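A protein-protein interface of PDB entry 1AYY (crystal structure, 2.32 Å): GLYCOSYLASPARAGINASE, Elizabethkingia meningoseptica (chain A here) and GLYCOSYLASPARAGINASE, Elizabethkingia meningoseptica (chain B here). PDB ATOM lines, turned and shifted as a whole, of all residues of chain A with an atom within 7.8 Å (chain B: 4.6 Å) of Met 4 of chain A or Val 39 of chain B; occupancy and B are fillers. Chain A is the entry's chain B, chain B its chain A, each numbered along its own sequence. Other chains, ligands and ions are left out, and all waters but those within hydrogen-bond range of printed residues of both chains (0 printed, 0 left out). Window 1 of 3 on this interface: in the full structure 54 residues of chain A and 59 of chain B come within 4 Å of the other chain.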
ATOM      1  N   THR A   1     -15.100 -13.722 -20.782  1.00  0.00           N
ATOM      2  CA  THR A   1     -16.265 -12.822 -20.553  1.00  0.00           C
ATOM      3  C   THR A   1     -15.960 -11.788 -19.481  1.00  0.00           C
ATOM      4  O   THR A   1     -15.370 -12.109 -18.447  1.00  0.00           O
ATOM      5  CB  THR A   1     -17.511 -13.610 -20.088  1.00  0.00           C
ATOM      6  OG1 THR A   1     -17.806 -14.650 -21.027  1.00  0.00           O
ATOM      7  CG2 THR A   1     -18.714 -12.684 -19.971  1.00  0.00           C
ATOM      8  N   ILE A   2     -16.359 -10.548 -19.736  1.00  0.00           N
ATOM      9  CA  ILE A   2     -16.164  -9.474 -18.770  1.00  0.00           C
ATOM     10  C   ILE A   2     -17.436  -8.640 -18.661  1.00  0.00           C
ATOM     11  O   ILE A   2     -17.863  -8.012 -19.628  1.00  0.00           O
ATOM     12  CB  ILE A   2     -14.987  -8.536 -19.148  1.00  0.00           C
ATOM     13  CG1 ILE A   2     -14.994  -7.308 -18.232  1.00  0.00           C
ATOM     14  CG2 ILE A   2     -15.106  -8.084 -20.597  1.00  0.00           C
ATOM     15  CD1 ILE A   2     -13.772  -7.181 -17.352  1.00  0.00           C
ATOM     16  N   GLY A   3     -18.044  -8.663 -17.481  1.00  0.00           N
ATOM     17  CA  GLY A   3     -19.245  -7.888 -17.242  1.00  0.00           C
ATOM     18  C   GLY A   3     -18.854  -6.751 -16.322  1.00  0.00           C
ATOM     19  O   GLY A   3     -18.127  -6.960 -15.351  1.00  0.00           O
ATOM     20  N   MET A   4     -19.321  -5.544 -16.623  1.00  0.00           N
ATOM     21  CA  MET A   4     -18.988  -4.381 -15.810  1.00  0.00           C
ATOM     22  C   MET A   4     -20.207  -3.503 -15.549  1.00  0.00           C
ATOM     23  O   MET A   4     -20.998  -3.239 -16.453  1.00  0.00           O
ATOM     24  CB  MET A   4     -17.893  -3.567 -16.511  1.00  0.00           C
ATOM     25  CG  MET A   4     -17.578  -2.223 -15.868  1.00  0.00           C
ATOM     26  SD  MET A   4     -16.070  -1.476 -16.545  1.00  0.00           S
ATOM     27  CE  MET A   4     -14.805  -2.446 -15.706  1.00  0.00           C
ATOM     28  N   ILE A   5     -20.350  -3.058 -14.304  1.00  0.00           N
ATOM     29  CA  ILE A   5     -21.457  -2.196 -13.897  1.00  0.00           C
ATOM     30  C   ILE A   5     -20.894  -1.096 -13.004  1.00  0.00           C
ATOM     31  O   ILE A   5     -19.946  -1.331 -12.254  1.00  0.00           O
ATOM     32  CB  ILE A   5     -22.533  -2.982 -13.111  1.00  0.00           C
ATOM     33  CG1 ILE A   5     -21.878  -3.809 -12.001  1.00  0.00           C
ATOM     34  CG2 ILE A   5     -23.308  -3.890 -14.057  1.00  0.00           C
ATOM     35  CD1 ILE A   5     -22.871  -4.506 -11.089  1.00  0.00           C
ATOM     36  N   ALA A   6     -21.468   0.100 -13.077  1.00  0.00           N
ATOM     37  CA  ALA A   6     -20.966   1.207 -12.271  1.00  0.00           C
ATOM     38  C   ALA A   6     -21.996   2.271 -11.912  1.00  0.00           C
ATOM     39  O   ALA A   6     -23.067   2.355 -12.508  1.00  0.00           O
ATOM     40  CB  ALA A   6     -19.789   1.861 -12.986  1.00  0.00           C
ATOM     41  N   SER A  14     -25.025   2.063 -15.059  1.00  0.00           N
ATOM     42  CA  SER A  14     -24.793   1.630 -16.429  1.00  0.00           C
ATOM     43  C   SER A  14     -24.039   0.310 -16.398  1.00  0.00           C
ATOM     44  O   SER A  14     -23.309   0.028 -15.448  1.00  0.00           O
ATOM     45  CB  SER A  14     -23.974   2.677 -17.193  1.00  0.00           C
ATOM     46  OG  SER A  14     -24.804   3.704 -17.710  1.00  0.00           O
ATOM     47  N   GLY A  15     -24.218  -0.497 -17.437  1.00  0.00           N
ATOM     48  CA  GLY A  15     -23.538  -1.776 -17.488  1.00  0.00           C
ATOM     49  C   GLY A  15     -22.994  -2.116 -18.860  1.00  0.00           C
ATOM     50  O   GLY A  15     -23.410  -1.548 -19.870  1.00  0.00           O
ATOM     51  N   ALA A  16     -22.057  -3.056 -18.893  1.00  0.00           N
ATOM     52  CA  ALA A  16     -21.449  -3.485 -20.139  1.00  0.00           C
ATOM     53  C   ALA A  16     -21.045  -4.949 -20.042  1.00  0.00           C
ATOM     54  O   ALA A  16     -20.424  -5.368 -19.070  1.00  0.00           O
ATOM     55  CB  ALA A  16     -20.231  -2.624 -20.452  1.00  0.00           C
ATOM     56  N   CYS A  17     -21.410  -5.727 -21.055  1.00  0.00           N
ATOM     57  CA  CYS A  17     -21.071  -7.143 -21.087  1.00  0.00           C
ATOM     58  C   CYS A  17     -20.625  -7.527 -22.489  1.00  0.00           C
ATOM     59  O   CYS A  17     -21.375  -7.373 -23.451  1.00  0.00           O
ATOM     60  CB  CYS A  17     -22.274  -7.996 -20.674  1.00  0.00           C
ATOM     61  SG  CYS A  17     -21.836  -9.678 -20.166  1.00  0.00           S
ATOM     62  N   THR A  18     -19.400  -8.022 -22.594  1.00  0.00           N
ATOM     63  CA  THR A  18     -18.840  -8.431 -23.877  1.00  0.00           C
ATOM     64  C   THR A  18     -18.125  -9.767 -23.691  1.00  0.00           C
ATOM     65  O   THR A  18     -17.552 -10.022 -22.635  1.00  0.00           O
ATOM     66  CB  THR A  18     -17.849  -7.365 -24.409  1.00  0.00           C
ATOM     67  OG1 THR A  18     -17.211  -7.846 -25.598  1.00  0.00           O
ATOM     68  CG2 THR A  18     -16.795  -7.046 -23.358  1.00  0.00           C
ATOM     69  N   THR A  19     -18.165 -10.621 -24.710  1.00  0.00           N
ATOM     70  CA  THR A  19     -17.524 -11.929 -24.614  1.00  0.00           C
ATOM     71  C   THR A  19     -17.304 -12.572 -25.975  1.00  0.00           C
ATOM     72  O   THR A  19     -17.781 -12.074 -26.993  1.00  0.00           O
ATOM     73  CB  THR A  19     -18.379 -12.902 -23.760  1.00  0.00           C
ATOM     74  OG1 THR A  19     -17.627 -14.088 -23.480  1.00  0.00           O
ATOM     75  CG2 THR A  19     -19.653 -13.288 -24.503  1.00  0.00           C
ATOM     76  N   GLY A  39     -27.657 -11.509 -19.446  1.00  0.00           N
ATOM     77  CA  GLY A  39     -26.288 -11.195 -19.085  1.00  0.00           C
ATOM     78  C   GLY A  39     -26.127  -9.810 -18.487  1.00  0.00           C
ATOM     79  O   GLY A  39     -25.091  -9.497 -17.906  1.00  0.00           O
ATOM     80  N   LEU A  40     -27.151  -8.974 -18.619  1.00  0.00           N
ATOM     81  CA  LEU A  40     -27.072  -7.624 -18.081  1.00  0.00           C
ATOM     82  C   LEU A  40     -28.414  -6.904 -18.012  1.00  0.00           C
ATOM     83  O   LEU A  40     -29.275  -7.069 -18.878  1.00  0.00           O
ATOM     84  CB  LEU A  40     -26.090  -6.796 -18.917  1.00  0.00           C
ATOM     85  CG  LEU A  40     -26.073  -5.284 -18.694  1.00  0.00           C
ATOM     86  CD1 LEU A  40     -25.228  -4.948 -17.470  1.00  0.00           C
ATOM     87  CD2 LEU A  40     -25.518  -4.601 -19.936  1.00  0.00           C
ATOM     88  N   VAL A  42     -30.017  -3.000 -16.157  1.00  0.00           N
ATOM     89  CA  VAL A  42     -29.824  -1.813 -15.338  1.00  0.00           C
ATOM     90  C   VAL A  42     -31.129  -1.057 -15.140  1.00  0.00           C
ATOM     91  O   VAL A  42     -31.913  -0.891 -16.072  1.00  0.00           O
ATOM     92  CB  VAL A  42     -28.804  -0.846 -15.986  1.00  0.00           C
ATOM     93  CG1 VAL A  42     -28.569   0.350 -15.078  1.00  0.00           C
ATOM     94  CG2 VAL A  42     -27.499  -1.569 -16.264  1.00  0.00           C
ATOM     95  N   ALA A  48     -28.042  -2.332 -10.698  1.00  0.00           N
ATOM     96  CA  ALA A  48     -27.592  -3.032 -11.893  1.00  0.00           C
ATOM     97  C   ALA A  48     -26.940  -4.366 -11.549  1.00  0.00           C
ATOM     98  O   ALA A  48     -26.471  -4.577 -10.431  1.00  0.00           O
ATOM     99  CB  ALA A  48     -26.608  -2.159 -12.669  1.00  0.00           C
ATOM    100  N   ALA A  49     -26.919  -5.266 -12.526  1.00  0.00           N
ATOM    101  CA  ALA A  49     -26.316  -6.576 -12.349  1.00  0.00           C
ATOM    102  C   ALA A  49     -25.861  -7.121 -13.697  1.00  0.00           C
ATOM    103  O   ALA A  49     -26.432  -6.796 -14.738  1.00  0.00           O
ATOM    104  CB  ALA A  49     -27.314  -7.531 -11.706  1.00  0.00           C
ATOM    105  N   THR A  50     -24.818  -7.941 -13.666  1.00  0.00           N
ATOM    106  CA  THR A  50     -24.273  -8.557 -14.866  1.00  0.00           C
ATOM    107  C   THR A  50     -23.754  -9.931 -14.462  1.00  0.00           C
ATOM    108  O   THR A  50     -23.357 -10.126 -13.315  1.00  0.00           O
ATOM    109  CB  THR A  50     -23.130  -7.708 -15.462  1.00  0.00           C
ATOM    110  OG1 THR A  50     -22.908  -8.098 -16.824  1.00  0.00           O
ATOM    111  CG2 THR A  50     -21.849  -7.898 -14.672  1.00  0.00           C
ATOM    112  N   ALA A  51     -23.762 -10.879 -15.393  1.00  0.00           N
ATOM    113  CA  ALA A  51     -23.314 -12.234 -15.088  1.00  0.00           C
ATOM    114  C   ALA A  51     -22.232 -12.758 -16.023  1.00  0.00           C
ATOM    115  O   ALA A  51     -21.898 -12.130 -17.028  1.00  0.00           O
ATOM    116  CB  ALA A  51     -24.506 -13.184 -15.102  1.00  0.00           C
ATOM    117  N   ILE A 107     -22.679 -10.278 -10.196  1.00  0.00           N
ATOM    118  CA  ILE A 107     -22.139  -9.157  -9.438  1.00  0.00           C
ATOM    119  C   ILE A 107     -23.241  -8.105  -9.499  1.00  0.00           C
ATOM    120  O   ILE A 107     -23.788  -7.841 -10.572  1.00  0.00           O
ATOM    121  CB  ILE A 107     -20.818  -8.606 -10.047  1.00  0.00           C
ATOM    122  CG1 ILE A 107     -21.044  -8.100 -11.471  1.00  0.00           C
ATOM    123  CG2 ILE A 107     -19.755  -9.691 -10.039  1.00  0.00           C
ATOM    124  CD1 ILE A 107     -19.858  -7.334 -12.034  1.00  0.00           C
ATOM    125  N   ALA A 127     -13.773  -7.578  -9.280  1.00  0.00           N
ATOM    126  CA  ALA A 127     -12.981  -6.402  -8.951  1.00  0.00           C
ATOM    127  C   ALA A 127     -13.882  -5.224  -8.623  1.00  0.00           C
ATOM    128  O   ALA A 127     -14.847  -4.950  -9.336  1.00  0.00           O
ATOM    129  CB  ALA A 127     -12.062  -6.052 -10.109  1.00  0.00           C
ATOM    130  N   VAL B   7     -17.208   1.061  -9.384  1.00  0.00           N
ATOM    131  CA  VAL B   7     -17.334   0.180 -10.540  1.00  0.00           C
ATOM    132  C   VAL B   7     -17.026  -1.276 -10.179  1.00  0.00           C
ATOM    133  O   VAL B   7     -16.173  -1.554  -9.333  1.00  0.00           O
ATOM    134  CB  VAL B   7     -16.404   0.650 -11.695  1.00  0.00           C
ATOM    135  CG1 VAL B   7     -15.022   0.988 -11.155  1.00  0.00           C
ATOM    136  CG2 VAL B   7     -16.312  -0.421 -12.772  1.00  0.00           C
ATOM    137  N   LEU B   8     -17.736  -2.200 -10.823  1.00  0.00           N
ATOM    138  CA  LEU B   8     -17.562  -3.629 -10.583  1.00  0.00           C
ATOM    139  C   LEU B   8     -17.416  -4.381 -11.904  1.00  0.00           C
ATOM    140  O   LEU B   8     -18.171  -4.140 -12.843  1.00  0.00           O
ATOM    141  CB  LEU B   8     -18.777  -4.188  -9.833  1.00  0.00           C
ATOM    142  CG  LEU B   8     -18.787  -4.209  -8.303  1.00  0.00           C
ATOM    143  CD1 LEU B   8     -19.914  -5.111  -7.821  1.00  0.00           C
ATOM    144  CD2 LEU B   8     -17.456  -4.708  -7.783  1.00  0.00           C
ATOM    145  N   SER B   9     -16.447  -5.292 -11.969  1.00  0.00           N
ATOM    146  CA  SER B   9     -16.221  -6.086 -13.175  1.00  0.00           C
ATOM    147  C   SER B   9     -15.832  -7.511 -12.796  1.00  0.00           C
ATOM    148  O   SER B   9     -15.208  -7.739 -11.761  1.00  0.00           O
ATOM    149  CB  SER B   9     -15.127  -5.456 -14.041  1.00  0.00           C
ATOM    150  OG  SER B   9     -13.876  -5.470 -13.378  1.00  0.00           O
ATOM    151  N   ALA B  17      -9.179  -3.596 -15.869  1.00  0.00           N
ATOM    152  CA  ALA B  17     -10.236  -3.006 -16.678  1.00  0.00           C
ATOM    153  C   ALA B  17     -10.944  -1.922 -15.877  1.00  0.00           C
ATOM    154  O   ALA B  17     -11.409  -0.933 -16.437  1.00  0.00           O
ATOM    155  CB  ALA B  17     -11.237  -4.073 -17.095  1.00  0.00           C
ATOM    156  N   ASN B  18     -11.025  -2.117 -14.562  1.00  0.00           N
ATOM    157  CA  ASN B  18     -11.678  -1.158 -13.673  1.00  0.00           C
ATOM    158  C   ASN B  18     -10.944   0.179 -13.664  1.00  0.00           C
ATOM    159  O   ASN B  18     -11.560   1.239 -13.515  1.00  0.00           O
ATOM    160  CB  ASN B  18     -11.728  -1.710 -12.246  1.00  0.00           C
ATOM    161  CG  ASN B  18     -12.982  -2.517 -11.972  1.00  0.00           C
ATOM    162  OD1 ASN B  18     -13.928  -2.504 -12.757  1.00  0.00           O
ATOM    163  ND2 ASN B  18     -12.992  -3.228 -10.851  1.00  0.00           N
ATOM    164  N   ALA B  21     -12.066   2.387 -16.399  1.00  0.00           N
ATOM    165  CA  ALA B  21     -13.405   2.898 -16.148  1.00  0.00           C
ATOM    166  C   ALA B  21     -13.330   4.018 -15.116  1.00  0.00           C
ATOM    167  O   ALA B  21     -14.014   5.036 -15.233  1.00  0.00           O
ATOM    168  CB  ALA B  21     -14.304   1.779 -15.639  1.00  0.00           C
ATOM    169  N   ALA B  34     -17.838   5.088 -19.019  1.00  0.00           N
ATOM    170  CA  ALA B  34     -16.916   4.384 -18.135  1.00  0.00           C
ATOM    171  C   ALA B  34     -16.931   2.877 -18.367  1.00  0.00           C
ATOM    172  O   ALA B  34     -15.876   2.250 -18.502  1.00  0.00           O
ATOM    173  CB  ALA B  34     -17.258   4.689 -16.681  1.00  0.00           C
ATOM    174  N   VAL B  35     -18.127   2.298 -18.411  1.00  0.00           N
ATOM    175  CA  VAL B  35     -18.266   0.860 -18.613  1.00  0.00           C
ATOM    176  C   VAL B  35     -17.873   0.424 -20.022  1.00  0.00           C
ATOM    177  O   VAL B  35     -17.643  -0.760 -20.271  1.00  0.00           O
ATOM    178  CB  VAL B  35     -19.713   0.391 -18.314  1.00  0.00           C
ATOM    179  CG1 VAL B  35     -20.082   0.750 -16.888  1.00  0.00           C
ATOM    180  CG2 VAL B  35     -20.692   1.027 -19.292  1.00  0.00           C
ATOM    181  N   GLU B  36     -17.798   1.378 -20.942  1.00  0.00           N
ATOM    182  CA  GLU B  36     -17.418   1.075 -22.315  1.00  0.00           C
ATOM    183  C   GLU B  36     -15.900   1.031 -22.426  1.00  0.00           C
ATOM    184  O   GLU B  36     -15.336   0.086 -22.975  1.00  0.00           O
ATOM    185  CB  GLU B  36     -17.981   2.135 -23.271  1.00  0.00           C
ATOM    186  CG  GLU B  36     -17.210   2.271 -24.578  1.00  0.00           C
ATOM    187  CD  GLU B  36     -17.962   3.072 -25.627  1.00  0.00           C
ATOM    188  OE1 GLU B  36     -18.487   4.153 -25.292  1.00  0.00           O
ATOM    189  OE2 GLU B  36     -18.028   2.617 -26.789  1.00  0.00           O
ATOM    190  N   LYS B  37     -15.242   2.057 -21.894  1.00  0.00           N
ATOM    191  CA  LYS B  37     -13.785   2.142 -21.937  1.00  0.00           C
ATOM    192  C   LYS B  37     -13.130   1.014 -21.145  1.00  0.00           C
ATOM    193  O   LYS B  37     -12.016   0.583 -21.455  1.00  0.00           O
ATOM    194  CB  LYS B  37     -13.320   3.490 -21.379  1.00  0.00           C
ATOM    195  CG  LYS B  37     -13.952   4.697 -22.057  1.00  0.00           C
ATOM    196  CD  LYS B  37     -12.934   5.487 -22.866  1.00  0.00           C
ATOM    197  CE  LYS B  37     -13.479   6.852 -23.283  1.00  0.00           C
ATOM    198  NZ  LYS B  37     -14.894   6.787 -23.752  1.00  0.00           N
ATOM    199  N   GLY B  38     -13.831   0.544 -20.119  1.00  0.00           N
ATOM    200  CA  GLY B  38     -13.304  -0.523 -19.292  1.00  0.00           C
ATOM    201  C   GLY B  38     -13.274  -1.882 -19.960  1.00  0.00           C
ATOM    202  O   GLY B  38     -12.213  -2.504 -20.041  1.00  0.00           O
ATOM    203  N   VAL B  39     -14.430  -2.348 -20.431  1.00  0.00           N
ATOM    204  CA  VAL B  39     -14.508  -3.654 -21.079  1.00  0.00           C
ATOM    205  C   VAL B  39     -13.736  -3.678 -22.387  1.00  0.00           C
ATOM    206  O   VAL B  39     -13.331  -4.742 -22.853  1.00  0.00           O
ATOM    207  CB  VAL B  39     -15.970  -4.079 -21.358  1.00  0.00           C
ATOM    208  CG1 VAL B  39     -16.741  -4.152 -20.052  1.00  0.00           C
ATOM    209  CG2 VAL B  39     -16.630  -3.107 -22.335  1.00  0.00           C
ATOM    210  N   ARG B  40     -13.537  -2.502 -22.976  1.00  0.00           N
ATOM    211  CA  ARG B  40     -12.809  -2.396 -24.238  1.00  0.00           C
ATOM    212  C   ARG B  40     -11.351  -2.771 -24.028  1.00  0.00           C
ATOM    213  O   ARG B  40     -10.695  -3.283 -24.936  1.00  0.00           O
ATOM    214  CB  ARG B  40     -12.901  -0.972 -24.792  1.00  0.00           C
ATOM    215  CG  ARG B  40     -14.081  -0.748 -25.726  1.00  0.00           C
ATOM    216  CD  ARG B  40     -14.103   0.678 -26.242  1.00  0.00           C
ATOM    217  NE  ARG B  40     -13.547   0.778 -27.588  1.00  0.00           N
ATOM    218  CZ  ARG B  40     -12.251   0.896 -27.852  1.00  0.00           C
ATOM    219  NH1 ARG B  40     -11.369   0.930 -26.862  1.00  0.00           N
ATOM    220  NH2 ARG B  40     -11.838   0.980 -29.108  1.00  0.00           N
ATOM    221  N   LEU B  41     -10.852  -2.518 -22.822  1.00  0.00           N
ATOM    222  CA  LEU B  41      -9.471  -2.839 -22.490  1.00  0.00           C
ATOM    223  C   LEU B  41      -9.242  -4.338 -22.651  1.00  0.00           C
ATOM    224  O   LEU B  41      -8.200  -4.762 -23.148  1.00  0.00           O
ATOM    225  CB  LEU B  41      -9.153  -2.417 -21.052  1.00  0.00           C
ATOM    226  CG  LEU B  41      -7.722  -2.719 -20.587  1.00  0.00           C
ATOM    227  CD1 LEU B  41      -6.730  -1.868 -21.377  1.00  0.00           C
ATOM    228  CD2 LEU B  41      -7.595  -2.442 -19.100  1.00  0.00           C
ATOM    229  N   VAL B  42     -10.226  -5.130 -22.234  1.00  0.00           N
ATOM    230  CA  VAL B  42     -10.141  -6.586 -22.324  1.00  0.00           C
ATOM    231  C   VAL B  42     -10.424  -7.079 -23.742  1.00  0.00           C
ATOM    232  O   VAL B  42     -10.018  -8.177 -24.118  1.00  0.00           O
ATOM    233  CB  VAL B  42     -11.135  -7.265 -21.357  1.00  0.00           C
ATOM    234  CG1 VAL B  42     -10.773  -8.734 -21.183  1.00  0.00           C
ATOM    235  CG2 VAL B  42     -11.118  -6.557 -20.013  1.00  0.00           C
ATOM    236  N   GLU B  43     -11.124  -6.266 -24.523  1.00  0.00           N
ATOM    237  CA  GLU B  43     -11.442  -6.624 -25.901  1.00  0.00           C
ATOM    238  C   GLU B  43     -10.185  -6.559 -26.768  1.00  0.00           C
ATOM    239  O   GLU B  43      -9.964  -7.420 -27.621  1.00  0.00           O
ATOM    240  CB  GLU B  43     -12.498  -5.671 -26.467  1.00  0.00           C
ATOM    241  CG  GLU B  43     -13.920  -6.004 -26.059  1.00  0.00           C
ATOM    242  CD  GLU B  43     -14.921  -4.977 -26.555  1.00  0.00           C
ATOM    243  OE1 GLU B  43     -14.488  -3.894 -27.007  1.00  0.00           O
ATOM    244  OE2 GLU B  43     -16.138  -5.254 -26.493  1.00  0.00           O
ATOM    245  N   ILE B  89     -18.619  -4.088 -28.103  1.00  0.00           N
ATOM    246  CA  ILE B  89     -19.291  -3.251 -27.116  1.00  0.00           C
ATOM    247  C   ILE B  89     -19.597  -1.869 -27.692  1.00  0.00           C
ATOM    248  O   ILE B  89     -20.594  -1.243 -27.333  1.00  0.00           O
ATOM    249  CB  ILE B  89     -18.433  -3.095 -25.831  1.00  0.00           C
ATOM    250  CG1 ILE B  89     -19.306  -2.582 -24.685  1.00  0.00           C
ATOM    251  CG2 ILE B  89     -17.275  -2.135 -26.074  1.00  0.00           C
ATOM    252  CD1 ILE B  89     -20.399  -3.550 -24.266  1.00  0.00           C
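Among the printed residues, merely in contact across the chains: Gly 3 of chain A with Ser 9 of chain B (3.0 Å), Ala 127 of chain A with Leu 8 of chain B (3.0 Å), Met 4 of chain A with Asn 18 of chain B (3.1 Å), Met 4 of chain A with Leu 8 of chain B (3.1 Å), Ala 16 of chain A with Val 35 of chain B (3.2 Å), Met 4 of chain A with Ser 9 of chain B (3.5 Å), Ile 5 of chain A with Val 7 of chain B (3.5 Å), Ser 14 of chain A with Val 35 of chain B (3.6 Å), Ala 127 of chain A with Val 7 of chain B (3.6 Å), Thr 18 of chain A with Val 39 of chain B (3.7 Å), Ile 107 of chain A with Leu 8 of chain B (3.7 Å), Met 4 of chain A with Val 39 of chain B (3.8 Å), Gly 3 of chain A with Leu 8 of chain B (3.8 Å), Gly 15 of chain A with Val 35 of chain B (3.8 Å), Met 4 of chain A with Ala 17 of chain B (3.8 Å), Met 4 of chain A with Val 7 of chain B (3.8 Å), Ile 2 of chain A with Val 42 of chain B (3.8 Å), Met 4 of chain A with Ala 21 of chain B (3.8 Å), Met 4 of chain A with Val 35 of chain B (3.8 Å), Ala 6 of chain A with Val 7 of chain B (3.8 Å), Ala 16 of chain A with Val 39 of chain B (3.8 Å), Ala 16 of chain A with Ile 89 of chain B (3.9 Å), Ile 2 of chain A with Ser 9 of chain B (3.97 Å) and Ile 107 of chain A with Ser 9 of chain B (3.98 Å).
The backbone NH (N) of Ala 127 of chain A is in hydrogen-bond range of the backbone carbonyl oxygen (O) of Ser 9 of chain B. O of Ala 127 of chain A is in hydrogen-bond range of ND2 of Asn 18 of chain B. OE2 of Glu 43 of chain B lies within hydrogen-bond range of OG1 of Thr 18 of chain A (2.9 Å). The backbone carbonyl oxygen of Ile 5 of chain A lies within hydrogen-bond range of the backbone NH of Leu 8 of chain B (2.8 Å).
Of chain A, only Met 4 (3.8 Å), Ala 16 (3.8 Å) and Thr 18 (3.7 Å) come within 4 Å of Val 39 of chain B. Of the printed residues of chain B, Gly 15 of chain A touches Val 35. Printed residues of chain B within 4 Å of Ile 107 of chain A: Leu 8 (3.7 Å) and Ser 9 (3.98 Å). Of the printed residues of chain A, Val 7 of chain B touches Met 4 (3.8 Å), Ile 5 (3.5 Å), Ala 6 (3.8 Å) and Ala 127 (3.6 Å). Thr 1 of chain A touches none of the printed residues of chain B. Ala 49 of chain A touches none of the printed residues of chain B. The nearest printed residue of chain B that does not touch Met 4 of chain A is Gly 38 of chain B (4.01 Å).
Hydrophobic or aromatic side chains of chain B within 4 Å of the printed part of chain A: Val 7, Leu 8, Ala 21, Val 35, Val 39, Val 42 and Ile 89. Hydrophobic or aromatic side chains of chain A within 4 Å of the printed part of chain B: Ile 2, Met 4, Ile 5, Ala 6, Ala 16, Ile 107 and Ala 127. Among the printed residues, no Asp or Glu carboxylate lies within 4 Å of a Lys or Arg side-chain nitrogen of the other chain.
The backbone carbonyl oxygen (O) of Thr 50 of chain A lies within hydrogen-bond range of the backbone NH (N) of Ile 107 of chain A, at 3.2 Å. OG of Ser 9 of chain B is in hydrogen-bond range of OD1 of Asn 18 of chain B (3.0 Å). O of Met 4 of chain A is in hydrogen-bond range of N of Ala 16 of chain A (2.7 Å). N of Ile 2 of chain A sits at hydrogen-bond distance from O of Thr 18 of chain A (3.2 Å). The side-chain carboxylate (OE2) of Glu 43 of chain B lies within hydrogen-bond range of the backbone NH (N) of Ile 89 of chain B, at 3.2 Å. The backbone NH (N) of Ala 6 of chain A lies within hydrogen-bond range of the backbone carbonyl oxygen (O) of Ser 14 of chain A (3.0 Å).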
